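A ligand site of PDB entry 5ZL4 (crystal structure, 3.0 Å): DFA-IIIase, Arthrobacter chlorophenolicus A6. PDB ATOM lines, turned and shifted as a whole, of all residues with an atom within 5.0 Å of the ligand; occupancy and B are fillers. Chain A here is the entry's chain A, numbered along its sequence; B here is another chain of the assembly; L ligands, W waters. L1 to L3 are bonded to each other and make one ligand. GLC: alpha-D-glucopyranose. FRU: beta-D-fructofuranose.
O of Pro 257 is in hydrogen-bond range of O4 of FRU L3.
The side-chain carboxylate (OE2) of Glu 210 lies within hydrogen-bond range of an oxygen (O3) of FRU L3 (2.7 Å).
The guanidinium group (NH1) of Arg 134 of chain B lies within hydrogen-bond range of an oxygen (O4) of FRU L2 (3.1 Å).
NH1 of Arg 258 is in hydrogen-bond range of O5 of FRU L3, 3.2 Å away.
OG of Ser 84 touches C1 of FRU L3, 3.8 Å away.
Ile 85 touches the ligand.
CA of Gly 232 touches O4 of FRU L3 (3.99 Å).
Phe 256 touches the ligand.
CE2 of Phe 281 touches O6 of FRU L3, at 3.4 Å.
CG of Pro 308 touches O3 of GLC L1 (3.6 Å).
Trp 309 touches the ligand.
Asp 177 of chain B touches the ligand.
CB of Asp 199 of chain B touches O4 of FRU L2, at 3.7 Å.
CG of Gln 222 of chain B touches C6 of GLC L1, 3.6 Å away.
CB of Ala 223 of chain B touches O6 of FRU L2 (3.7 Å).
The side-chain carboxylate of Glu 210 sits at hydrogen-bond distance from the backbone NH of Ser 84, 3.0 Å away.
The backbone NH (N) of Glu 210 is in hydrogen-bond range of the backbone carbonyl oxygen (O) of Gly 232 (3.2 Å).
NH2 of Arg 134 of chain B lies within salt-bridge range of OD2 of Asp 177 of chain B.
The backbone NH of Arg 258 sits at hydrogen-bond distance from the backbone carbonyl oxygen of Ala 233, 2.8 Å away.
The side-chain hydroxyl (OH) of Tyr 163 lies within hydrogen-bond range of the guanidinium group (NH1) of Arg 258 (3.3 Å).
The side-chain carboxylate (OE1) of Glu 307 lies within salt-bridge range of the guanidinium group (NE) of Arg 258 (2.9 Å).
N of Gln 222 of chain B sits close to OD1 of Asp 199 of chain B, at 3.4 Å.
N of Ile 85 lies within hydrogen-bond range of OG of Ser 82 (3.1 Å).
Water W1 lies within hydrogen-bond range of O4 of FRU L3 (2.7 Å), O of Ala 233 (2.7 Å), OH of Tyr 163 (2.8 Å), N of Glu 210 (3.2 Å) and O of Gly 232 (3.4 Å).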
ATOM      1  N   PHE A  80     -39.238  13.213  23.408  1.00  0.00           N
ATOM      2  CA  PHE A  80     -37.847  12.921  23.058  1.00  0.00           C
ATOM      3  C   PHE A  80     -37.098  12.298  24.247  1.00  0.00           C
ATOM      4  O   PHE A  80     -37.111  12.836  25.347  1.00  0.00           O
ATOM      5  CB  PHE A  80     -37.105  14.182  22.603  1.00  0.00           C
ATOM      6  CG  PHE A  80     -35.654  13.942  22.268  1.00  0.00           C
ATOM      7  CD1 PHE A  80     -34.681  14.027  23.255  1.00  0.00           C
ATOM      8  CD2 PHE A  80     -35.270  13.605  20.979  1.00  0.00           C
ATOM      9  CE1 PHE A  80     -33.344  13.796  22.964  1.00  0.00           C
ATOM     10  CE2 PHE A  80     -33.941  13.364  20.682  1.00  0.00           C
ATOM     11  CZ  PHE A  80     -32.982  13.459  21.672  1.00  0.00           C
ATOM     12  N   SER A  82     -32.994  10.336  24.291  1.00  0.00           N
ATOM     13  CA  SER A  82     -31.826  10.130  23.404  1.00  0.00           C
ATOM     14  C   SER A  82     -31.596   8.661  23.033  1.00  0.00           C
ATOM     15  O   SER A  82     -30.850   7.961  23.728  1.00  0.00           O
ATOM     16  CB  SER A  82     -30.558  10.720  24.025  1.00  0.00           C
ATOM     17  OG  SER A  82     -29.403  10.349  23.277  1.00  0.00           O
ATOM     18  N   SER A  84     -29.812   7.676  20.613  1.00  0.00           N
ATOM     19  CA  SER A  84     -28.378   7.577  20.348  1.00  0.00           C
ATOM     20  C   SER A  84     -27.602   7.126  21.575  1.00  0.00           C
ATOM     21  O   SER A  84     -26.819   6.189  21.492  1.00  0.00           O
ATOM     22  CB  SER A  84     -27.832   8.913  19.856  1.00  0.00           C
ATOM     23  OG  SER A  84     -26.437   8.835  19.612  1.00  0.00           O
ATOM     24  N   ILE A  85     -27.840   7.771  22.715  1.00  0.00           N
ATOM     25  CA  ILE A  85     -27.157   7.388  23.951  1.00  0.00           C
ATOM     26  C   ILE A  85     -27.447   5.932  24.303  1.00  0.00           C
ATOM     27  O   ILE A  85     -26.515   5.159  24.509  1.00  0.00           O
ATOM     28  CB  ILE A  85     -27.471   8.352  25.130  1.00  0.00           C
ATOM     29  CG1 ILE A  85     -26.562   9.589  25.003  1.00  0.00           C
ATOM     30  CG2 ILE A  85     -27.242   7.684  26.488  1.00  0.00           C
ATOM     31  CD1 ILE A  85     -27.006  10.798  25.801  1.00  0.00           C
ATOM     32  N   TYR A 163     -26.886   7.418  11.021  1.00  0.00           N
ATOM     33  CA  TYR A 163     -27.884   8.436  10.681  1.00  0.00           C
ATOM     34  C   TYR A 163     -28.553   8.134   9.325  1.00  0.00           C
ATOM     35  O   TYR A 163     -28.823   9.042   8.535  1.00  0.00           O
ATOM     36  CB  TYR A 163     -27.288   9.851  10.703  1.00  0.00           C
ATOM     37  CG  TYR A 163     -26.962  10.425  12.066  1.00  0.00           C
ATOM     38  CD1 TYR A 163     -27.929  11.120  12.800  1.00  0.00           C
ATOM     39  CD2 TYR A 163     -25.671  10.352  12.607  1.00  0.00           C
ATOM     40  CE1 TYR A 163     -27.636  11.689  14.033  1.00  0.00           C
ATOM     41  CE2 TYR A 163     -25.363  10.921  13.837  1.00  0.00           C
ATOM     42  CZ  TYR A 163     -26.342  11.585  14.553  1.00  0.00           C
ATOM     43  OH  TYR A 163     -26.056  12.154  15.780  1.00  0.00           O
ATOM     44  N   ALA A 209     -33.792  16.473  17.012  1.00  0.00           N
ATOM     45  CA  ALA A 209     -32.469  15.953  17.355  1.00  0.00           C
ATOM     46  C   ALA A 209     -32.276  14.502  16.947  1.00  0.00           C
ATOM     47  O   ALA A 209     -33.247  13.765  16.793  1.00  0.00           O
ATOM     48  CB  ALA A 209     -32.214  16.110  18.835  1.00  0.00           C
ATOM     49  N   GLU A 210     -31.000  14.124  16.811  1.00  0.00           N
ATOM     50  CA  GLU A 210     -30.595  12.769  16.423  1.00  0.00           C
ATOM     51  C   GLU A 210     -31.296  12.319  15.143  1.00  0.00           C
ATOM     52  O   GLU A 210     -31.833  11.203  15.047  1.00  0.00           O
ATOM     53  CB  GLU A 210     -30.773  11.805  17.599  1.00  0.00           C
ATOM     54  CG  GLU A 210     -29.816  12.105  18.740  1.00  0.00           C
ATOM     55  CD  GLU A 210     -30.175  11.421  20.042  1.00  0.00           C
ATOM     56  OE1 GLU A 210     -30.905  10.403  19.995  1.00  0.00           O
ATOM     57  OE2 GLU A 210     -29.710  11.899  21.114  1.00  0.00           O
ATOM     58  N   GLY A 232     -30.185  19.325  16.470  1.00  0.00           N
ATOM     59  CA  GLY A 232     -28.967  18.528  16.412  1.00  0.00           C
ATOM     60  C   GLY A 232     -29.101  17.516  15.294  1.00  0.00           C
ATOM     61  O   GLY A 232     -30.064  16.753  15.255  1.00  0.00           O
ATOM     62  N   ALA A 233     -28.128  17.506  14.381  1.00  0.00           N
ATOM     63  CA  ALA A 233     -28.180  16.624  13.221  1.00  0.00           C
ATOM     64  C   ALA A 233     -27.007  15.628  13.208  1.00  0.00           C
ATOM     65  O   ALA A 233     -26.311  15.468  14.231  1.00  0.00           O
ATOM     66  CB  ALA A 233     -28.212  17.470  11.954  1.00  0.00           C
ATOM     67  N   PHE A 256     -27.031  22.509  18.327  1.00  0.00           N
ATOM     68  CA  PHE A 256     -25.908  21.732  18.878  1.00  0.00           C
ATOM     69  C   PHE A 256     -25.418  20.725  17.818  1.00  0.00           C
ATOM     70  O   PHE A 256     -26.014  20.635  16.735  1.00  0.00           O
ATOM     71  CB  PHE A 256     -26.284  21.070  20.241  1.00  0.00           C
ATOM     72  CG  PHE A 256     -27.635  20.412  20.288  1.00  0.00           C
ATOM     73  CD1 PHE A 256     -27.789  19.076  19.959  1.00  0.00           C
ATOM     74  CD2 PHE A 256     -28.761  21.112  20.700  1.00  0.00           C
ATOM     75  CE1 PHE A 256     -29.021  18.451  20.025  1.00  0.00           C
ATOM     76  CE2 PHE A 256     -30.001  20.507  20.759  1.00  0.00           C
ATOM     77  CZ  PHE A 256     -30.136  19.182  20.419  1.00  0.00           C
ATOM     78  N   PRO A 257     -24.302  20.008  18.087  1.00  0.00           N
ATOM     79  CA  PRO A 257     -23.819  19.034  17.106  1.00  0.00           C
ATOM     80  C   PRO A 257     -24.823  17.891  16.829  1.00  0.00           C
ATOM     81  O   PRO A 257     -25.792  17.756  17.567  1.00  0.00           O
ATOM     82  CB  PRO A 257     -22.527  18.504  17.765  1.00  0.00           C
ATOM     83  CG  PRO A 257     -22.078  19.634  18.621  1.00  0.00           C
ATOM     84  CD  PRO A 257     -23.332  20.206  19.178  1.00  0.00           C
ATOM     85  N   ARG A 258     -24.609  17.060  15.809  1.00  0.00           N
ATOM     86  CA  ARG A 258     -23.385  16.970  15.030  1.00  0.00           C
ATOM     87  C   ARG A 258     -23.675  16.992  13.535  1.00  0.00           C
ATOM     88  O   ARG A 258     -23.211  16.136  12.792  1.00  0.00           O
ATOM     89  CB  ARG A 258     -22.596  15.709  15.427  1.00  0.00           C
ATOM     90  CG  ARG A 258     -23.372  14.400  15.379  1.00  0.00           C
ATOM     91  CD  ARG A 258     -22.473  13.231  15.752  1.00  0.00           C
ATOM     92  NE  ARG A 258     -21.973  13.359  17.119  1.00  0.00           N
ATOM     93  CZ  ARG A 258     -22.627  12.993  18.229  1.00  0.00           C
ATOM     94  NH1 ARG A 258     -23.844  12.444  18.159  1.00  0.00           N
ATOM     95  NH2 ARG A 258     -22.056  13.186  19.415  1.00  0.00           N
ATOM     96  N   PHE A 281     -18.888  20.325  16.074  1.00  0.00           N
ATOM     97  CA  PHE A 281     -17.598  19.690  16.276  1.00  0.00           C
ATOM     98  C   PHE A 281     -16.707  19.756  15.030  1.00  0.00           C
ATOM     99  O   PHE A 281     -15.584  19.261  15.058  1.00  0.00           O
ATOM    100  CB  PHE A 281     -17.778  18.220  16.715  1.00  0.00           C
ATOM    101  CG  PHE A 281     -18.470  18.041  18.049  1.00  0.00           C
ATOM    102  CD1 PHE A 281     -18.139  18.817  19.158  1.00  0.00           C
ATOM    103  CD2 PHE A 281     -19.424  17.025  18.212  1.00  0.00           C
ATOM    104  CE1 PHE A 281     -18.758  18.615  20.385  1.00  0.00           C
ATOM    105  CE2 PHE A 281     -20.057  16.823  19.441  1.00  0.00           C
ATOM    106  CZ  PHE A 281     -19.724  17.619  20.528  1.00  0.00           C
ATOM    107  N   GLU A 307     -15.209  16.861  19.246  1.00  0.00           N
ATOM    108  CA  GLU A 307     -16.133  15.839  19.779  1.00  0.00           C
ATOM    109  C   GLU A 307     -15.527  15.144  21.006  1.00  0.00           C
ATOM    110  O   GLU A 307     -14.430  14.603  20.896  1.00  0.00           O
ATOM    111  CB  GLU A 307     -16.406  14.795  18.690  1.00  0.00           C
ATOM    112  CG  GLU A 307     -17.140  13.544  19.150  1.00  0.00           C
ATOM    113  CD  GLU A 307     -18.639  13.722  19.166  1.00  0.00           C
ATOM    114  OE1 GLU A 307     -19.225  13.701  18.063  1.00  0.00           O
ATOM    115  OE2 GLU A 307     -19.229  13.857  20.272  1.00  0.00           O
ATOM    116  N   PRO A 308     -16.236  15.128  22.156  1.00  0.00           N
ATOM    117  CA  PRO A 308     -15.729  14.429  23.353  1.00  0.00           C
ATOM    118  C   PRO A 308     -16.281  13.013  23.553  1.00  0.00           C
ATOM    119  O   PRO A 308     -15.705  12.242  24.327  1.00  0.00           O
ATOM    120  CB  PRO A 308     -16.202  15.319  24.486  1.00  0.00           C
ATOM    121  CG  PRO A 308     -17.516  15.825  24.005  1.00  0.00           C
ATOM    122  CD  PRO A 308     -17.419  15.935  22.503  1.00  0.00           C
ATOM    123  N   TRP A 309     -17.396  12.696  22.884  1.00  0.00           N
ATOM    124  CA  TRP A 309     -18.080  11.437  23.089  1.00  0.00           C
ATOM    125  C   TRP A 309     -17.406  10.342  22.263  1.00  0.00           C
ATOM    126  O   TRP A 309     -17.383  10.411  21.037  1.00  0.00           O
ATOM    127  CB  TRP A 309     -19.563  11.572  22.706  1.00  0.00           C
ATOM    128  CG  TRP A 309     -20.420  10.471  23.250  1.00  0.00           C
ATOM    129  CD1 TRP A 309     -20.295   9.845  24.454  1.00  0.00           C
ATOM    130  CD2 TRP A 309     -21.554   9.864  22.611  1.00  0.00           C
ATOM    131  NE1 TRP A 309     -21.262   8.888  24.596  1.00  0.00           N
ATOM    132  CE2 TRP A 309     -22.050   8.883  23.490  1.00  0.00           C
ATOM    133  CE3 TRP A 309     -22.197  10.068  21.381  1.00  0.00           C
ATOM    134  CZ2 TRP A 309     -23.167   8.088  23.179  1.00  0.00           C
ATOM    135  CZ3 TRP A 309     -23.292   9.284  21.072  1.00  0.00           C
ATOM    136  CH2 TRP A 309     -23.764   8.303  21.968  1.00  0.00           C
ATOM    137  N   ARG B 134     -31.383   9.939  31.807  1.00  0.00           N
ATOM    138  CA  ARG B 134     -31.918  11.178  32.362  1.00  0.00           C
ATOM    139  C   ARG B 134     -33.436  11.218  32.163  1.00  0.00           C
ATOM    140  O   ARG B 134     -33.942  10.821  31.110  1.00  0.00           O
ATOM    141  CB  ARG B 134     -31.281  12.400  31.705  1.00  0.00           C
ATOM    142  CG  ARG B 134     -29.789  12.561  31.967  1.00  0.00           C
ATOM    143  CD  ARG B 134     -29.173  13.521  30.964  1.00  0.00           C
ATOM    144  NE  ARG B 134     -29.153  12.954  29.605  1.00  0.00           N
ATOM    145  CZ  ARG B 134     -28.925  13.641  28.480  1.00  0.00           C
ATOM    146  NH1 ARG B 134     -28.701  14.958  28.507  1.00  0.00           N
ATOM    147  NH2 ARG B 134     -28.940  13.009  27.303  1.00  0.00           N
ATOM    148  N   ASP B 177     -33.289  15.938  30.494  1.00  0.00           N
ATOM    149  CA  ASP B 177     -33.012  16.185  29.073  1.00  0.00           C
ATOM    150  C   ASP B 177     -34.334  16.554  28.397  1.00  0.00           C
ATOM    151  O   ASP B 177     -35.343  15.900  28.637  1.00  0.00           O
ATOM    152  CB  ASP B 177     -32.395  14.925  28.416  1.00  0.00           C
ATOM    153  CG  ASP B 177     -31.876  15.157  26.977  1.00  0.00           C
ATOM    154  OD1 ASP B 177     -31.501  16.292  26.592  1.00  0.00           O
ATOM    155  OD2 ASP B 177     -31.801  14.152  26.230  1.00  0.00           O
ATOM    156  N   ASP B 199     -30.229  19.616  30.749  1.00  0.00           N
ATOM    157  CA  ASP B 199     -29.736  19.529  29.371  1.00  0.00           C
ATOM    158  C   ASP B 199     -30.886  19.780  28.391  1.00  0.00           C
ATOM    159  O   ASP B 199     -31.970  19.232  28.555  1.00  0.00           O
ATOM    160  CB  ASP B 199     -29.110  18.153  29.120  1.00  0.00           C
ATOM    161  CG  ASP B 199     -27.830  17.938  29.922  1.00  0.00           C
ATOM    162  OD1 ASP B 199     -27.013  18.878  29.969  1.00  0.00           O
ATOM    163  OD2 ASP B 199     -27.630  16.840  30.487  1.00  0.00           O
ATOM    164  N   GLN B 222     -26.444  22.223  29.994  1.00  0.00           N
ATOM    165  CA  GLN B 222     -25.960  22.377  28.630  1.00  0.00           C
ATOM    166  C   GLN B 222     -27.076  22.629  27.636  1.00  0.00           C
ATOM    167  O   GLN B 222     -28.177  22.069  27.753  1.00  0.00           O
ATOM    168  CB  GLN B 222     -25.235  21.107  28.190  1.00  0.00           C
ATOM    169  CG  GLN B 222     -23.886  20.879  28.870  1.00  0.00           C
ATOM    170  CD  GLN B 222     -22.820  21.890  28.504  1.00  0.00           C
ATOM    171  OE1 GLN B 222     -21.909  22.147  29.303  1.00  0.00           O
ATOM    172  NE2 GLN B 222     -22.903  22.487  27.293  1.00  0.00           N
ATOM    173  N   ALA B 223     -26.774  23.472  26.642  1.00  0.00           N
ATOM    174  CA  ALA B 223     -27.577  23.643  25.438  1.00  0.00           C
ATOM    175  C   ALA B 223     -29.050  23.981  25.709  1.00  0.00           C
ATOM    176  O   ALA B 223     -29.930  23.537  24.984  1.00  0.00           O
ATOM    177  CB  ALA B 223     -27.457  22.395  24.569  1.00  0.00           C
HETATM  178  C1  GLC L   1     -22.707  16.083  24.603  1.00  0.00           C
HETATM  179  C2  GLC L   1     -21.498  15.181  24.673  1.00  0.00           C
HETATM  180  C3  GLC L   1     -21.138  14.838  26.101  1.00  0.00           C
HETATM  181  C4  GLC L   1     -20.991  16.091  26.932  1.00  0.00           C
HETATM  182  C5  GLC L   1     -22.181  16.999  26.743  1.00  0.00           C
HETATM  183  C6  GLC L   1     -21.848  18.357  27.324  1.00  0.00           C
HETATM  184  O2  GLC L   1     -21.792  13.971  24.006  1.00  0.00           O
HETATM  185  O3  GLC L   1     -19.904  14.115  26.123  1.00  0.00           O
HETATM  186  O4  GLC L   1     -20.852  15.720  28.297  1.00  0.00           O
HETATM  187  O5  GLC L   1     -22.475  17.226  25.386  1.00  0.00           O
HETATM  188  O6  GLC L   1     -20.859  18.981  26.506  1.00  0.00           O
HETATM  189  C1  FRU L   2     -24.853  14.446  23.150  1.00  0.00           C
HETATM  190  C2  FRU L   2     -24.987  15.443  24.292  1.00  0.00           C
HETATM  191  C3  FRU L   2     -26.194  15.145  25.126  1.00  0.00           C
HETATM  192  C4  FRU L   2     -26.549  16.497  25.656  1.00  0.00           C
HETATM  193  C5  FRU L   2     -26.239  17.394  24.486  1.00  0.00           C
HETATM  194  C6  FRU L   2     -25.927  18.817  24.931  1.00  0.00           C
HETATM  195  O1  FRU L   2     -26.096  14.275  22.465  1.00  0.00           O
HETATM  196  O2  FRU L   2     -23.842  15.416  25.120  1.00  0.00           O
HETATM  197  O3  FRU L   2     -25.927  14.237  26.191  1.00  0.00           O
HETATM  198  O4  FRU L   2     -27.922  16.570  26.011  1.00  0.00           O
HETATM  199  O5  FRU L   2     -25.134  16.765  23.830  1.00  0.00           O
HETATM  200  O6  FRU L   2     -25.163  19.500  23.924  1.00  0.00           O
HETATM  201  C1  FRU L   3     -25.881  12.253  21.144  1.00  0.00           C
HETATM  202  C2  FRU L   3     -25.961  13.742  21.146  1.00  0.00           C
HETATM  203  C3  FRU L   3     -27.117  14.148  20.291  1.00  0.00           C
HETATM  204  C4  FRU L   3     -26.690  15.481  19.780  1.00  0.00           C
HETATM  205  C5  FRU L   3     -25.181  15.476  19.864  1.00  0.00           C
HETATM  206  C6  FRU L   3     -24.607  16.598  20.695  1.00  0.00           C
HETATM  207  O1  FRU L   3     -24.883  11.966  22.084  1.00  0.00           O
HETATM  208  O3  FRU L   3     -28.308  14.168  21.045  1.00  0.00           O
HETATM  209  O4  FRU L   3     -27.096  15.636  18.433  1.00  0.00           O
HETATM  210  O5  FRU L   3     -24.823  14.296  20.524  1.00  0.00           O
HETATM  211  O6  FRU L   3     -23.210  16.410  20.744  1.00  0.00           O
HETATM  212  O   HOH W   1     -27.852  14.321  16.195  1.00  0.00           O
HETATM  213  O   HOH W   2     -24.221  21.645  23.129  1.00  0.00           O
HETATM  214  O   HOH W   3     -29.793  15.802  23.497  1.00  0.00           O
